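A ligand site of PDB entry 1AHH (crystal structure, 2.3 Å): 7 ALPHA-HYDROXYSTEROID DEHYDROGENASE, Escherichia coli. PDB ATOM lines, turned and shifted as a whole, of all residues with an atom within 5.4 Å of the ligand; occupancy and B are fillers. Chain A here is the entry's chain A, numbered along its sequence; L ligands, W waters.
Water W1 lies within hydrogen-bond range of O of Ala 21 (2.5 Å), O9 of the ligand (2.7 Å), N of Gly 24 (2.8 Å), ND2 of Asn 95 (3.0 Å) and O of Gly 18 (3.2 Å).
Water W2 bridges an oxygen (O6) of the ligand (3.0 Å) and the side-chain amide oxygen (OD1) of Asn 44 (3.4 Å).
The backbone carbonyl oxygen (O) of Asp 42 lies within hydrogen-bond range of the backbone NH (N) of Cys 67, 3.1 Å away.
The backbone NH of Asn 44 is in hydrogen-bond range of the side-chain carboxylate of Asp 42.
The side-chain amino group (NZ) of Lys 163 sits at hydrogen-bond distance from the side-chain amide oxygen (OD1) of Asn 118 (2.9 Å).
ND2 of Asn 95 sits at hydrogen-bond distance from O of Gly 18, 2.6 Å away.
OD1 of Asp 68 sits at hydrogen-bond distance from OG1 of Thr 70, at 2.7 Å.
The backbone NH of Gly 18 is in hydrogen-bond range of the backbone carbonyl oxygen of Ser 41 (2.9 Å).
The side-chain hydroxyl (OH) of Tyr 159 is in hydrogen-bond range of the side-chain hydroxyl (OG) of Ser 146 (3.1 Å).
The side-chain amide nitrogen of Asn 118 is in hydrogen-bond range of the backbone carbonyl oxygen of Gly 98 (2.7 Å).
The backbone carbonyl oxygen (O) of Cys 67 sits close to a nitrogen (N4) of the ligand (3.2 Å).
O of Gly 190 sits close to O14 of the ligand (3.4 Å).
Merely in contact with the ligand: Thr 145 (3.2 Å), Ile 144 (3.3 Å), Gly 18 (3.4 Å), Gly 97 (3.4 Å), Pro 189 (3.5 Å), Tyr 159 (3.5 Å), Gly 98 (3.6 Å), Thr 194 (3.6 Å), Ser 146 (3.7 Å), Ala 191 (3.8 Å), Ala 96 (3.8 Å), Gly 20 (3.8 Å), Leu 197 (3.9 Å), Gly 22 (3.9 Å) and Leu 117 (3.9 Å).
Hydrophobic or aromatic side chains within 4 Å of the ligand: Ala 21, Ile 43, Ile 69, Leu 117, Ile 144, Tyr 159, Pro 189, Ile 192 and Leu 197.
26 residues have an atom within 4 Å of the ligand: Gly 18, Gly 20, Ala 21, Gly 22, Ile 23, Asp 42, Ile 43, Cys 67, Asp 68, Ile 69, Asn 95, Ala 96, Gly 97, Gly 98, Leu 117, Ile 144, Thr 145, Ser 146, Tyr 159, Lys 163, Pro 189, Gly 190, Ala 191, Ile 192, Thr 194 and Leu 197.
The side-chain carboxylate of Asp 42 sits at hydrogen-bond distance from an oxygen (O5) of the ligand (2.7 Å).
NZ of Lys 163 lies within hydrogen-bond range of O13 of the ligand, 2.9 Å away.
The backbone NH (N) of Ile 192 is in hydrogen-bond range of an oxygen (O14) of the ligand, at 2.9 Å.
An oxygen (O12) of the ligand sits at hydrogen-bond distance from the backbone carbonyl oxygen (O) of Asn 95 (3.0 Å).
N of Ile 69 sits at hydrogen-bond distance from N4 of the ligand.
OD1 of Asp 68 sits at hydrogen-bond distance from N3 of the ligand (3.1 Å).
N5 of the ligand is in hydrogen-bond range of N of Ile 43, 3.4 Å away.
The backbone NH (N) of Ala 21 is in hydrogen-bond range of an oxygen (O5) of the ligand, at 3.3 Å.
The backbone NH of Ile 23 lies within hydrogen-bond range of an oxygen (O9) of the ligand, 3.5 Å away.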
ATOM      1  N   GLY A  18      -8.103 -15.122   9.780  1.00  0.00           N
ATOM      2  CA  GLY A  18      -8.277 -15.620   8.424  1.00  0.00           C
ATOM      3  C   GLY A  18      -8.011 -14.557   7.384  1.00  0.00           C
ATOM      4  O   GLY A  18      -8.714 -14.457   6.377  1.00  0.00           O
ATOM      5  N   ALA A  19      -6.937 -13.798   7.578  1.00  0.00           N
ATOM      6  CA  ALA A  19      -6.608 -12.713   6.655  1.00  0.00           C
ATOM      7  C   ALA A  19      -5.604 -13.031   5.568  1.00  0.00           C
ATOM      8  O   ALA A  19      -5.168 -12.133   4.857  1.00  0.00           O
ATOM      9  CB  ALA A  19      -6.171 -11.500   7.422  1.00  0.00           C
ATOM     10  N   GLY A  20      -5.284 -14.304   5.396  1.00  0.00           N
ATOM     11  CA  GLY A  20      -4.310 -14.694   4.391  1.00  0.00           C
ATOM     12  C   GLY A  20      -4.835 -14.647   2.977  1.00  0.00           C
ATOM     13  O   GLY A  20      -4.062 -14.700   2.008  1.00  0.00           O
ATOM     14  N   ALA A  21      -6.150 -14.570   2.856  1.00  0.00           N
ATOM     15  CA  ALA A  21      -6.787 -14.509   1.562  1.00  0.00           C
ATOM     16  C   ALA A  21      -8.210 -13.990   1.636  1.00  0.00           C
ATOM     17  O   ALA A  21      -8.797 -13.878   2.720  1.00  0.00           O
ATOM     18  CB  ALA A  21      -6.789 -15.880   0.941  1.00  0.00           C
ATOM     19  N   GLY A  22      -8.738 -13.680   0.458  1.00  0.00           N
ATOM     20  CA  GLY A  22     -10.105 -13.204   0.315  1.00  0.00           C
ATOM     21  C   GLY A  22     -10.417 -11.913   1.016  1.00  0.00           C
ATOM     22  O   GLY A  22      -9.557 -11.034   1.136  1.00  0.00           O
ATOM     23  N   ILE A  23     -11.669 -11.792   1.446  1.00  0.00           N
ATOM     24  CA  ILE A  23     -12.165 -10.612   2.154  1.00  0.00           C
ATOM     25  C   ILE A  23     -11.206 -10.255   3.275  1.00  0.00           C
ATOM     26  O   ILE A  23     -10.868  -9.078   3.455  1.00  0.00           O
ATOM     27  CB  ILE A  23     -13.544 -10.892   2.775  1.00  0.00           C
ATOM     28  CG1 ILE A  23     -14.613 -10.979   1.683  1.00  0.00           C
ATOM     29  CG2 ILE A  23     -13.876  -9.832   3.792  1.00  0.00           C
ATOM     30  CD1 ILE A  23     -15.954 -11.382   2.233  1.00  0.00           C
ATOM     31  N   GLY A  24     -10.737 -11.268   3.998  1.00  0.00           N
ATOM     32  CA  GLY A  24      -9.819 -11.088   5.105  1.00  0.00           C
ATOM     33  C   GLY A  24      -8.533 -10.388   4.705  1.00  0.00           C
ATOM     34  O   GLY A  24      -8.030  -9.546   5.460  1.00  0.00           O
ATOM     35  N   SER A  41      -3.530 -13.321  10.827  1.00  0.00           N
ATOM     36  CA  SER A  41      -3.672 -14.715  11.227  1.00  0.00           C
ATOM     37  C   SER A  41      -4.317 -15.559  10.131  1.00  0.00           C
ATOM     38  O   SER A  41      -5.199 -15.097   9.418  1.00  0.00           O
ATOM     39  CB  SER A  41      -4.532 -14.782  12.480  1.00  0.00           C
ATOM     40  OG  SER A  41      -5.011 -16.101  12.697  1.00  0.00           O
ATOM     41  N   ASP A  42      -3.866 -16.801  10.013  1.00  0.00           N
ATOM     42  CA  ASP A  42      -4.384 -17.729   9.018  1.00  0.00           C
ATOM     43  C   ASP A  42      -3.749 -19.112   9.219  1.00  0.00           C
ATOM     44  O   ASP A  42      -2.656 -19.241   9.788  1.00  0.00           O
ATOM     45  CB  ASP A  42      -4.060 -17.221   7.605  1.00  0.00           C
ATOM     46  CG  ASP A  42      -5.054 -17.708   6.567  1.00  0.00           C
ATOM     47  OD1 ASP A  42      -4.879 -18.822   6.024  1.00  0.00           O
ATOM     48  OD2 ASP A  42      -6.013 -16.974   6.282  1.00  0.00           O
ATOM     49  N   ILE A  43      -4.461 -20.158   8.823  1.00  0.00           N
ATOM     50  CA  ILE A  43      -3.937 -21.494   8.946  1.00  0.00           C
ATOM     51  C   ILE A  43      -2.859 -21.712   7.882  1.00  0.00           C
ATOM     52  O   ILE A  43      -1.871 -22.399   8.111  1.00  0.00           O
ATOM     53  CB  ILE A  43      -5.043 -22.545   8.802  1.00  0.00           C
ATOM     54  CG1 ILE A  43      -5.804 -22.643  10.118  1.00  0.00           C
ATOM     55  CG2 ILE A  43      -4.474 -23.902   8.469  1.00  0.00           C
ATOM     56  CD1 ILE A  43      -6.598 -23.921  10.258  1.00  0.00           C
ATOM     57  N   ASN A  44      -3.025 -21.091   6.723  1.00  0.00           N
ATOM     58  CA  ASN A  44      -2.044 -21.228   5.659  1.00  0.00           C
ATOM     59  C   ASN A  44      -0.934 -20.172   5.763  1.00  0.00           C
ATOM     60  O   ASN A  44      -0.937 -19.166   5.056  1.00  0.00           O
ATOM     61  CB  ASN A  44      -2.736 -21.151   4.295  1.00  0.00           C
ATOM     62  CG  ASN A  44      -1.776 -21.313   3.134  1.00  0.00           C
ATOM     63  OD1 ASN A  44      -2.033 -20.835   2.037  1.00  0.00           O
ATOM     64  ND2 ASN A  44      -0.660 -21.999   3.368  1.00  0.00           N
ATOM     65  N   ALA A  47       0.372 -17.984   3.042  1.00  0.00           N
ATOM     66  CA  ALA A  47      -0.570 -16.944   2.632  1.00  0.00           C
ATOM     67  C   ALA A  47      -0.452 -15.767   3.583  1.00  0.00           C
ATOM     68  O   ALA A  47      -0.253 -14.641   3.142  1.00  0.00           O
ATOM     69  CB  ALA A  47      -1.980 -17.473   2.657  1.00  0.00           C
ATOM     70  N   CYS A  67      -2.655 -19.762  12.875  1.00  0.00           N
ATOM     71  CA  CYS A  67      -3.568 -20.014  13.949  1.00  0.00           C
ATOM     72  C   CYS A  67      -4.850 -20.618  13.467  1.00  0.00           C
ATOM     73  O   CYS A  67      -5.561 -20.041  12.645  1.00  0.00           O
ATOM     74  CB  CYS A  67      -3.917 -18.745  14.726  1.00  0.00           C
ATOM     75  SG  CYS A  67      -5.440 -18.923  15.742  1.00  0.00           S
ATOM     76  N   ASP A  68      -5.122 -21.813  13.971  1.00  0.00           N
ATOM     77  CA  ASP A  68      -6.339 -22.502  13.650  1.00  0.00           C
ATOM     78  C   ASP A  68      -7.301 -21.888  14.655  1.00  0.00           C
ATOM     79  O   ASP A  68      -7.107 -22.002  15.874  1.00  0.00           O
ATOM     80  CB  ASP A  68      -6.189 -24.008  13.880  1.00  0.00           C
ATOM     81  CG  ASP A  68      -7.459 -24.792  13.519  1.00  0.00           C
ATOM     82  OD1 ASP A  68      -8.497 -24.170  13.239  1.00  0.00           O
ATOM     83  OD2 ASP A  68      -7.413 -26.046  13.526  1.00  0.00           O
ATOM     84  N   ILE A  69      -8.275 -21.147  14.145  1.00  0.00           N
ATOM     85  CA  ILE A  69      -9.268 -20.525  14.999  1.00  0.00           C
ATOM     86  C   ILE A  69     -10.095 -21.547  15.782  1.00  0.00           C
ATOM     87  O   ILE A  69     -10.702 -21.202  16.776  1.00  0.00           O
ATOM     88  CB  ILE A  69     -10.222 -19.642  14.194  1.00  0.00           C
ATOM     89  CG1 ILE A  69     -10.992 -20.500  13.189  1.00  0.00           C
ATOM     90  CG2 ILE A  69      -9.423 -18.576  13.483  1.00  0.00           C
ATOM     91  CD1 ILE A  69     -12.223 -19.848  12.604  1.00  0.00           C
ATOM     92  N   THR A  70     -10.140 -22.802  15.334  1.00  0.00           N
ATOM     93  CA  THR A  70     -10.922 -23.821  16.034  1.00  0.00           C
ATOM     94  C   THR A  70     -10.209 -24.482  17.211  1.00  0.00           C
ATOM     95  O   THR A  70     -10.808 -25.294  17.933  1.00  0.00           O
ATOM     96  CB  THR A  70     -11.453 -24.907  15.080  1.00  0.00           C
ATOM     97  OG1 THR A  70     -10.365 -25.617  14.488  1.00  0.00           O
ATOM     98  CG2 THR A  70     -12.290 -24.274  13.992  1.00  0.00           C
ATOM     99  N   ASN A  95     -12.851 -12.590  10.988  1.00  0.00           N
ATOM    100  CA  ASN A  95     -13.178 -12.903   9.601  1.00  0.00           C
ATOM    101  C   ASN A  95     -13.302 -14.393   9.277  1.00  0.00           C
ATOM    102  O   ASN A  95     -14.253 -14.825   8.632  1.00  0.00           O
ATOM    103  CB  ASN A  95     -12.145 -12.265   8.665  1.00  0.00           C
ATOM    104  CG  ASN A  95     -12.143 -12.866   7.274  1.00  0.00           C
ATOM    105  OD1 ASN A  95     -13.037 -12.584   6.452  1.00  0.00           O
ATOM    106  ND2 ASN A  95     -11.174 -13.712   7.001  1.00  0.00           N
ATOM    107  N   ALA A  96     -12.312 -15.177   9.699  1.00  0.00           N
ATOM    108  CA  ALA A  96     -12.345 -16.599   9.434  1.00  0.00           C
ATOM    109  C   ALA A  96     -13.652 -17.220   9.878  1.00  0.00           C
ATOM    110  O   ALA A  96     -14.305 -16.751  10.811  1.00  0.00           O
ATOM    111  CB  ALA A  96     -11.176 -17.314  10.112  1.00  0.00           C
ATOM    112  N   GLY A  97     -14.041 -18.264   9.181  1.00  0.00           N
ATOM    113  CA  GLY A  97     -15.254 -18.946   9.515  1.00  0.00           C
ATOM    114  C   GLY A  97     -15.623 -19.691   8.268  1.00  0.00           C
ATOM    115  O   GLY A  97     -14.753 -19.944   7.431  1.00  0.00           O
ATOM    116  N   GLY A  98     -16.900 -20.040   8.140  1.00  0.00           N
ATOM    117  CA  GLY A  98     -17.331 -20.751   6.952  1.00  0.00           C
ATOM    118  C   GLY A  98     -18.405 -21.793   7.158  1.00  0.00           C
ATOM    119  O   GLY A  98     -19.412 -21.567   7.846  1.00  0.00           O
ATOM    120  N   ARG A 113     -19.051 -28.832  13.512  1.00  0.00           N
ATOM    121  CA  ARG A 113     -17.957 -28.054  12.934  1.00  0.00           C
ATOM    122  C   ARG A 113     -18.305 -26.606  12.573  1.00  0.00           C
ATOM    123  O   ARG A 113     -17.532 -25.680  12.845  1.00  0.00           O
ATOM    124  CB  ARG A 113     -17.426 -28.779  11.695  1.00  0.00           C
ATOM    125  CG  ARG A 113     -16.610 -27.905  10.765  1.00  0.00           C
ATOM    126  CD  ARG A 113     -15.121 -28.252  10.761  1.00  0.00           C
ATOM    127  NE  ARG A 113     -14.414 -27.923  12.004  1.00  0.00           N
ATOM    128  CZ  ARG A 113     -13.146 -27.506  12.042  1.00  0.00           C
ATOM    129  NH1 ARG A 113     -12.464 -27.313  10.913  1.00  0.00           N
ATOM    130  NH2 ARG A 113     -12.558 -27.247  13.209  1.00  0.00           N
ATOM    131  N   LEU A 117     -16.274 -23.051  13.868  1.00  0.00           N
ATOM    132  CA  LEU A 117     -15.796 -21.992  13.008  1.00  0.00           C
ATOM    133  C   LEU A 117     -16.504 -20.653  13.181  1.00  0.00           C
ATOM    134  O   LEU A 117     -15.881 -19.642  13.481  1.00  0.00           O
ATOM    135  CB  LEU A 117     -15.918 -22.448  11.552  1.00  0.00           C
ATOM    136  CG  LEU A 117     -15.012 -23.587  11.090  1.00  0.00           C
ATOM    137  CD1 LEU A 117     -15.414 -23.994   9.694  1.00  0.00           C
ATOM    138  CD2 LEU A 117     -13.551 -23.138  11.124  1.00  0.00           C
ATOM    139  N   ASN A 118     -17.819 -20.666  12.982  1.00  0.00           N
ATOM    140  CA  ASN A 118     -18.654 -19.475  13.058  1.00  0.00           C
ATOM    141  C   ASN A 118     -19.047 -18.959  14.435  1.00  0.00           C
ATOM    142  O   ASN A 118     -19.272 -17.750  14.584  1.00  0.00           O
ATOM    143  CB  ASN A 118     -19.945 -19.720  12.297  1.00  0.00           C
ATOM    144  CG  ASN A 118     -19.710 -20.058  10.831  1.00  0.00           C
ATOM    145  OD1 ASN A 118     -18.872 -19.468  10.174  1.00  0.00           O
ATOM    146  ND2 ASN A 118     -20.453 -21.007  10.325  1.00  0.00           N
ATOM    147  N   ILE A 144     -17.404 -11.304  10.651  1.00  0.00           N
ATOM    148  CA  ILE A 144     -17.979 -11.362   9.332  1.00  0.00           C
ATOM    149  C   ILE A 144     -18.977 -12.505   9.392  1.00  0.00           C
ATOM    150  O   ILE A 144     -18.590 -13.632   9.698  1.00  0.00           O
ATOM    151  CB  ILE A 144     -16.927 -11.643   8.285  1.00  0.00           C
ATOM    152  CG1 ILE A 144     -15.883 -10.531   8.340  1.00  0.00           C
ATOM    153  CG2 ILE A 144     -17.563 -11.723   6.912  1.00  0.00           C
ATOM    154  CD1 ILE A 144     -16.471  -9.133   8.341  1.00  0.00           C
ATOM    155  N   THR A 145     -20.263 -12.207   9.257  1.00  0.00           N
ATOM    156  CA  THR A 145     -21.249 -13.271   9.285  1.00  0.00           C
ATOM    157  C   THR A 145     -21.635 -13.709   7.863  1.00  0.00           C
ATOM    158  O   THR A 145     -20.788 -14.100   7.075  1.00  0.00           O
ATOM    159  CB  THR A 145     -22.488 -12.944  10.173  1.00  0.00           C
ATOM    160  OG1 THR A 145     -23.177 -11.799   9.655  1.00  0.00           O
ATOM    161  CG2 THR A 145     -22.046 -12.622  11.599  1.00  0.00           C
ATOM    162  N   SER A 146     -22.908 -13.610   7.513  1.00  0.00           N
ATOM    163  CA  SER A 146     -23.336 -14.040   6.208  1.00  0.00           C
ATOM    164  C   SER A 146     -24.826 -13.782   6.073  1.00  0.00           C
ATOM    165  O   SER A 146     -25.522 -13.601   7.078  1.00  0.00           O
ATOM    166  CB  SER A 146     -23.076 -15.517   6.049  1.00  0.00           C
ATOM    167  OG  SER A 146     -23.800 -16.025   4.948  1.00  0.00           O
ATOM    168  N   MET A 147     -25.309 -13.819   4.850  1.00  0.00           N
ATOM    169  CA  MET A 147     -26.717 -13.574   4.616  1.00  0.00           C
ATOM    170  C   MET A 147     -27.553 -14.781   4.939  1.00  0.00           C
ATOM    171  O   MET A 147     -28.780 -14.698   5.026  1.00  0.00           O
ATOM    172  CB  MET A 147     -26.950 -13.128   3.189  1.00  0.00           C
ATOM    173  CG  MET A 147     -26.451 -11.736   2.935  1.00  0.00           C
ATOM    174  SD  MET A 147     -26.902 -11.286   1.259  1.00  0.00           S
ATOM    175  CE  MET A 147     -28.666 -10.773   1.596  1.00  0.00           C
ATOM    176  N   TYR A 159     -24.745 -24.233   8.310  1.00  0.00           N
ATOM    177  CA  TYR A 159     -24.193 -22.944   7.963  1.00  0.00           C
ATOM    178  C   TYR A 159     -25.148 -21.834   8.373  1.00  0.00           C
ATOM    179  O   TYR A 159     -24.788 -20.965   9.172  1.00  0.00           O
ATOM    180  CB  TYR A 159     -23.945 -22.893   6.453  1.00  0.00           C
ATOM    181  CG  TYR A 159     -23.312 -21.608   5.997  1.00  0.00           C
ATOM    182  CD1 TYR A 159     -22.145 -21.140   6.583  1.00  0.00           C
ATOM    183  CD2 TYR A 159     -23.871 -20.869   4.969  1.00  0.00           C
ATOM    184  CE1 TYR A 159     -21.544 -19.963   6.147  1.00  0.00           C
ATOM    185  CE2 TYR A 159     -23.291 -19.708   4.523  1.00  0.00           C
ATOM    186  CZ  TYR A 159     -22.123 -19.254   5.108  1.00  0.00           C
ATOM    187  OH  TYR A 159     -21.498 -18.134   4.590  1.00  0.00           O
ATOM    188  N   LYS A 163     -24.365 -19.134  11.451  1.00  0.00           N
ATOM    189  CA  LYS A 163     -24.242 -17.721  11.164  1.00  0.00           C
ATOM    190  C   LYS A 163     -25.296 -16.907  11.921  1.00  0.00           C
ATOM    191  O   LYS A 163     -25.051 -15.802  12.341  1.00  0.00           O
ATOM    192  CB  LYS A 163     -24.359 -17.503   9.668  1.00  0.00           C
ATOM    193  CG  LYS A 163     -23.186 -18.066   8.919  1.00  0.00           C
ATOM    194  CD  LYS A 163     -21.885 -17.477   9.423  1.00  0.00           C
ATOM    195  CE  LYS A 163     -20.770 -17.607   8.386  1.00  0.00           C
ATOM    196  NZ  LYS A 163     -19.516 -16.923   8.841  1.00  0.00           N
ATOM    197  N   PRO A 189     -21.643 -10.377   4.289  1.00  0.00           N
ATOM    198  CA  PRO A 189     -21.308 -10.278   2.877  1.00  0.00           C
ATOM    199  C   PRO A 189     -22.320 -10.974   1.994  1.00  0.00           C
ATOM    200  O   PRO A 189     -22.941 -11.947   2.391  1.00  0.00           O
ATOM    201  CB  PRO A 189     -19.970 -10.994   2.797  1.00  0.00           C
ATOM    202  CG  PRO A 189     -19.371 -10.804   4.177  1.00  0.00           C
ATOM    203  CD  PRO A 189     -20.573 -11.038   5.054  1.00  0.00           C
ATOM    204  N   GLY A 190     -22.512 -10.425   0.802  1.00  0.00           N
ATOM    205  CA  GLY A 190     -23.383 -11.047  -0.183  1.00  0.00           C
ATOM    206  C   GLY A 190     -22.445 -11.960  -0.958  1.00  0.00           C
ATOM    207  O   GLY A 190     -21.496 -12.503  -0.385  1.00  0.00           O
ATOM    208  N   ALA A 191     -22.628 -12.114  -2.258  1.00  0.00           N
ATOM    209  CA  ALA A 191     -21.751 -13.001  -3.024  1.00  0.00           C
ATOM    210  C   ALA A 191     -20.480 -12.279  -3.387  1.00  0.00           C
ATOM    211  O   ALA A 191     -20.385 -11.641  -4.428  1.00  0.00           O
ATOM    212  CB  ALA A 191     -22.446 -13.522  -4.272  1.00  0.00           C
ATOM    213  N   ILE A 192     -19.495 -12.361  -2.513  1.00  0.00           N
ATOM    214  CA  ILE A 192     -18.246 -11.685  -2.775  1.00  0.00           C
ATOM    215  C   ILE A 192     -17.404 -12.493  -3.736  1.00  0.00           C
ATOM    216  O   ILE A 192     -17.169 -13.668  -3.531  1.00  0.00           O
ATOM    217  CB  ILE A 192     -17.448 -11.423  -1.477  1.00  0.00           C
ATOM    218  CG1 ILE A 192     -18.310 -10.634  -0.501  1.00  0.00           C
ATOM    219  CG2 ILE A 192     -16.193 -10.654  -1.776  1.00  0.00           C
ATOM    220  CD1 ILE A 192     -19.106  -9.523  -1.141  1.00  0.00           C
ATOM    221  N   LEU A 193     -16.980 -11.837  -4.807  1.00  0.00           N
ATOM    222  CA  LEU A 193     -16.144 -12.475  -5.808  1.00  0.00           C
ATOM    223  C   LEU A 193     -14.715 -12.547  -5.285  1.00  0.00           C
ATOM    224  O   LEU A 193     -13.817 -11.828  -5.771  1.00  0.00           O
ATOM    225  CB  LEU A 193     -16.204 -11.650  -7.100  1.00  0.00           C
ATOM    226  CG  LEU A 193     -15.659 -12.214  -8.405  1.00  0.00           C
ATOM    227  CD1 LEU A 193     -16.404 -13.497  -8.773  1.00  0.00           C
ATOM    228  CD2 LEU A 193     -15.803 -11.173  -9.515  1.00  0.00           C
ATOM    229  N   THR A 194     -14.499 -13.334  -4.230  1.00  0.00           N
ATOM    230  CA  THR A 194     -13.162 -13.506  -3.694  1.00  0.00           C
ATOM    231  C   THR A 194     -12.434 -14.259  -4.805  1.00  0.00           C
ATOM    232  O   THR A 194     -13.063 -15.025  -5.551  1.00  0.00           O
ATOM    233  CB  THR A 194     -13.167 -14.326  -2.391  1.00  0.00           C
ATOM    234  OG1 THR A 194     -14.124 -15.393  -2.483  1.00  0.00           O
ATOM    235  CG2 THR A 194     -13.518 -13.426  -1.216  1.00  0.00           C
ATOM    236  N   ALA A 196     -11.187 -16.865  -5.312  1.00  0.00           N
ATOM    237  CA  ALA A 196     -11.620 -18.250  -5.479  1.00  0.00           C
ATOM    238  C   ALA A 196     -12.837 -18.312  -6.411  1.00  0.00           C
ATOM    239  O   ALA A 196     -12.787 -18.904  -7.489  1.00  0.00           O
ATOM    240  CB  ALA A 196     -11.946 -18.879  -4.131  1.00  0.00           C
ATOM    241  N   LEU A 197     -13.934 -17.680  -6.002  1.00  0.00           N
ATOM    242  CA  LEU A 197     -15.147 -17.677  -6.823  1.00  0.00           C
ATOM    243  C   LEU A 197     -14.770 -17.127  -8.174  1.00  0.00           C
ATOM    244  O   LEU A 197     -15.124 -17.698  -9.202  1.00  0.00           O
ATOM    245  CB  LEU A 197     -16.232 -16.807  -6.189  1.00  0.00           C
ATOM    246  CG  LEU A 197     -16.566 -17.052  -4.710  1.00  0.00           C
ATOM    247  CD1 LEU A 197     -17.943 -16.465  -4.393  1.00  0.00           C
ATOM    248  CD2 LEU A 197     -16.532 -18.553  -4.418  1.00  0.00           C
HETATM  249  P1  LIG L   1     -11.967 -18.206   2.198  1.00  0.00           P
HETATM  250  O1  LIG L   1     -12.126 -19.657   2.522  1.00  0.00           O
HETATM  251  O2  LIG L   1     -11.660 -17.795   0.794  1.00  0.00           O
HETATM  252  O3  LIG L   1     -10.767 -17.616   3.088  1.00  0.00           O
HETATM  253  C1  LIG L   1     -10.696 -17.934   4.478  1.00  0.00           C
HETATM  254  C2  LIG L   1      -9.296 -17.565   4.902  1.00  0.00           C
HETATM  255  O4  LIG L   1      -9.193 -18.094   6.235  1.00  0.00           O
HETATM  256  C3  LIG L   1      -8.278 -18.291   4.037  1.00  0.00           C
HETATM  257  O5  LIG L   1      -7.050 -17.582   3.891  1.00  0.00           O
HETATM  258  C4  LIG L   1      -8.163 -19.623   4.761  1.00  0.00           C
HETATM  259  O6  LIG L   1      -6.886 -20.201   4.444  1.00  0.00           O
HETATM  260  C5  LIG L   1      -8.299 -19.200   6.218  1.00  0.00           C
HETATM  261  N1  LIG L   1      -8.815 -20.179   7.197  1.00  0.00           N
HETATM  262  C6  LIG L   1      -9.609 -21.258   6.971  1.00  0.00           C
HETATM  263  N2  LIG L   1      -9.822 -21.971   8.083  1.00  0.00           N
HETATM  264  C7  LIG L   1      -9.139 -21.292   8.997  1.00  0.00           C
HETATM  265  C8  LIG L   1      -9.031 -21.677  10.332  1.00  0.00           C
HETATM  266  N3  LIG L   1      -9.670 -22.783  10.737  1.00  0.00           N
HETATM  267  N4  LIG L   1      -8.265 -20.880  11.140  1.00  0.00           N
HETATM  268  C9  LIG L   1      -7.666 -19.788  10.639  1.00  0.00           C
HETATM  269  N5  LIG L   1      -7.771 -19.423   9.351  1.00  0.00           N
HETATM  270  C10 LIG L   1      -8.509 -20.167   8.500  1.00  0.00           C
HETATM  271  O7  LIG L   1     -13.263 -17.381   2.749  1.00  0.00           O
HETATM  272  P2  LIG L   1     -13.966 -15.919   2.588  1.00  0.00           P
HETATM  273  O8  LIG L   1     -14.976 -15.969   1.491  1.00  0.00           O
HETATM  274  O9  LIG L   1     -12.915 -14.874   2.449  1.00  0.00           O
HETATM  275  O10 LIG L   1     -14.835 -15.815   3.953  1.00  0.00           O
HETATM  276  C11 LIG L   1     -14.437 -15.206   5.174  1.00  0.00           C
HETATM  277  C12 LIG L   1     -15.727 -15.039   5.982  1.00  0.00           C
HETATM  278  O11 LIG L   1     -16.753 -14.410   5.171  1.00  0.00           O
HETATM  279  C13 LIG L   1     -16.302 -16.367   6.443  1.00  0.00           C
HETATM  280  O12 LIG L   1     -16.688 -16.304   7.824  1.00  0.00           O
HETATM  281  C14 LIG L   1     -17.492 -16.636   5.521  1.00  0.00           C
HETATM  282  O13 LIG L   1     -18.464 -17.444   6.232  1.00  0.00           O
HETATM  283  C15 LIG L   1     -17.953 -15.212   5.180  1.00  0.00           C
HETATM  284  N6  LIG L   1     -18.695 -15.051   3.894  1.00  0.00           N
HETATM  285  C16 LIG L   1     -18.106 -15.100   2.600  1.00  0.00           C
HETATM  286  C17 LIG L   1     -18.860 -14.932   1.410  1.00  0.00           C
HETATM  287  C18 LIG L   1     -18.291 -14.931  -0.066  1.00  0.00           C
HETATM  288  O14 LIG L   1     -19.073 -14.845  -1.040  1.00  0.00           O
HETATM  289  N7  LIG L   1     -16.960 -15.021  -0.268  1.00  0.00           N
HETATM  290  C19 LIG L   1     -20.242 -14.729   1.578  1.00  0.00           C
HETATM  291  C20 LIG L   1     -20.829 -14.691   2.846  1.00  0.00           C
HETATM  292  C21 LIG L   1     -20.060 -14.845   4.000  1.00  0.00           C
HETATM  293  O   HOH W   1     -10.870 -14.106   4.015  1.00  0.00           O
HETATM  294  O   HOH W   2      -5.095 -19.297   2.275  1.00  0.00           O
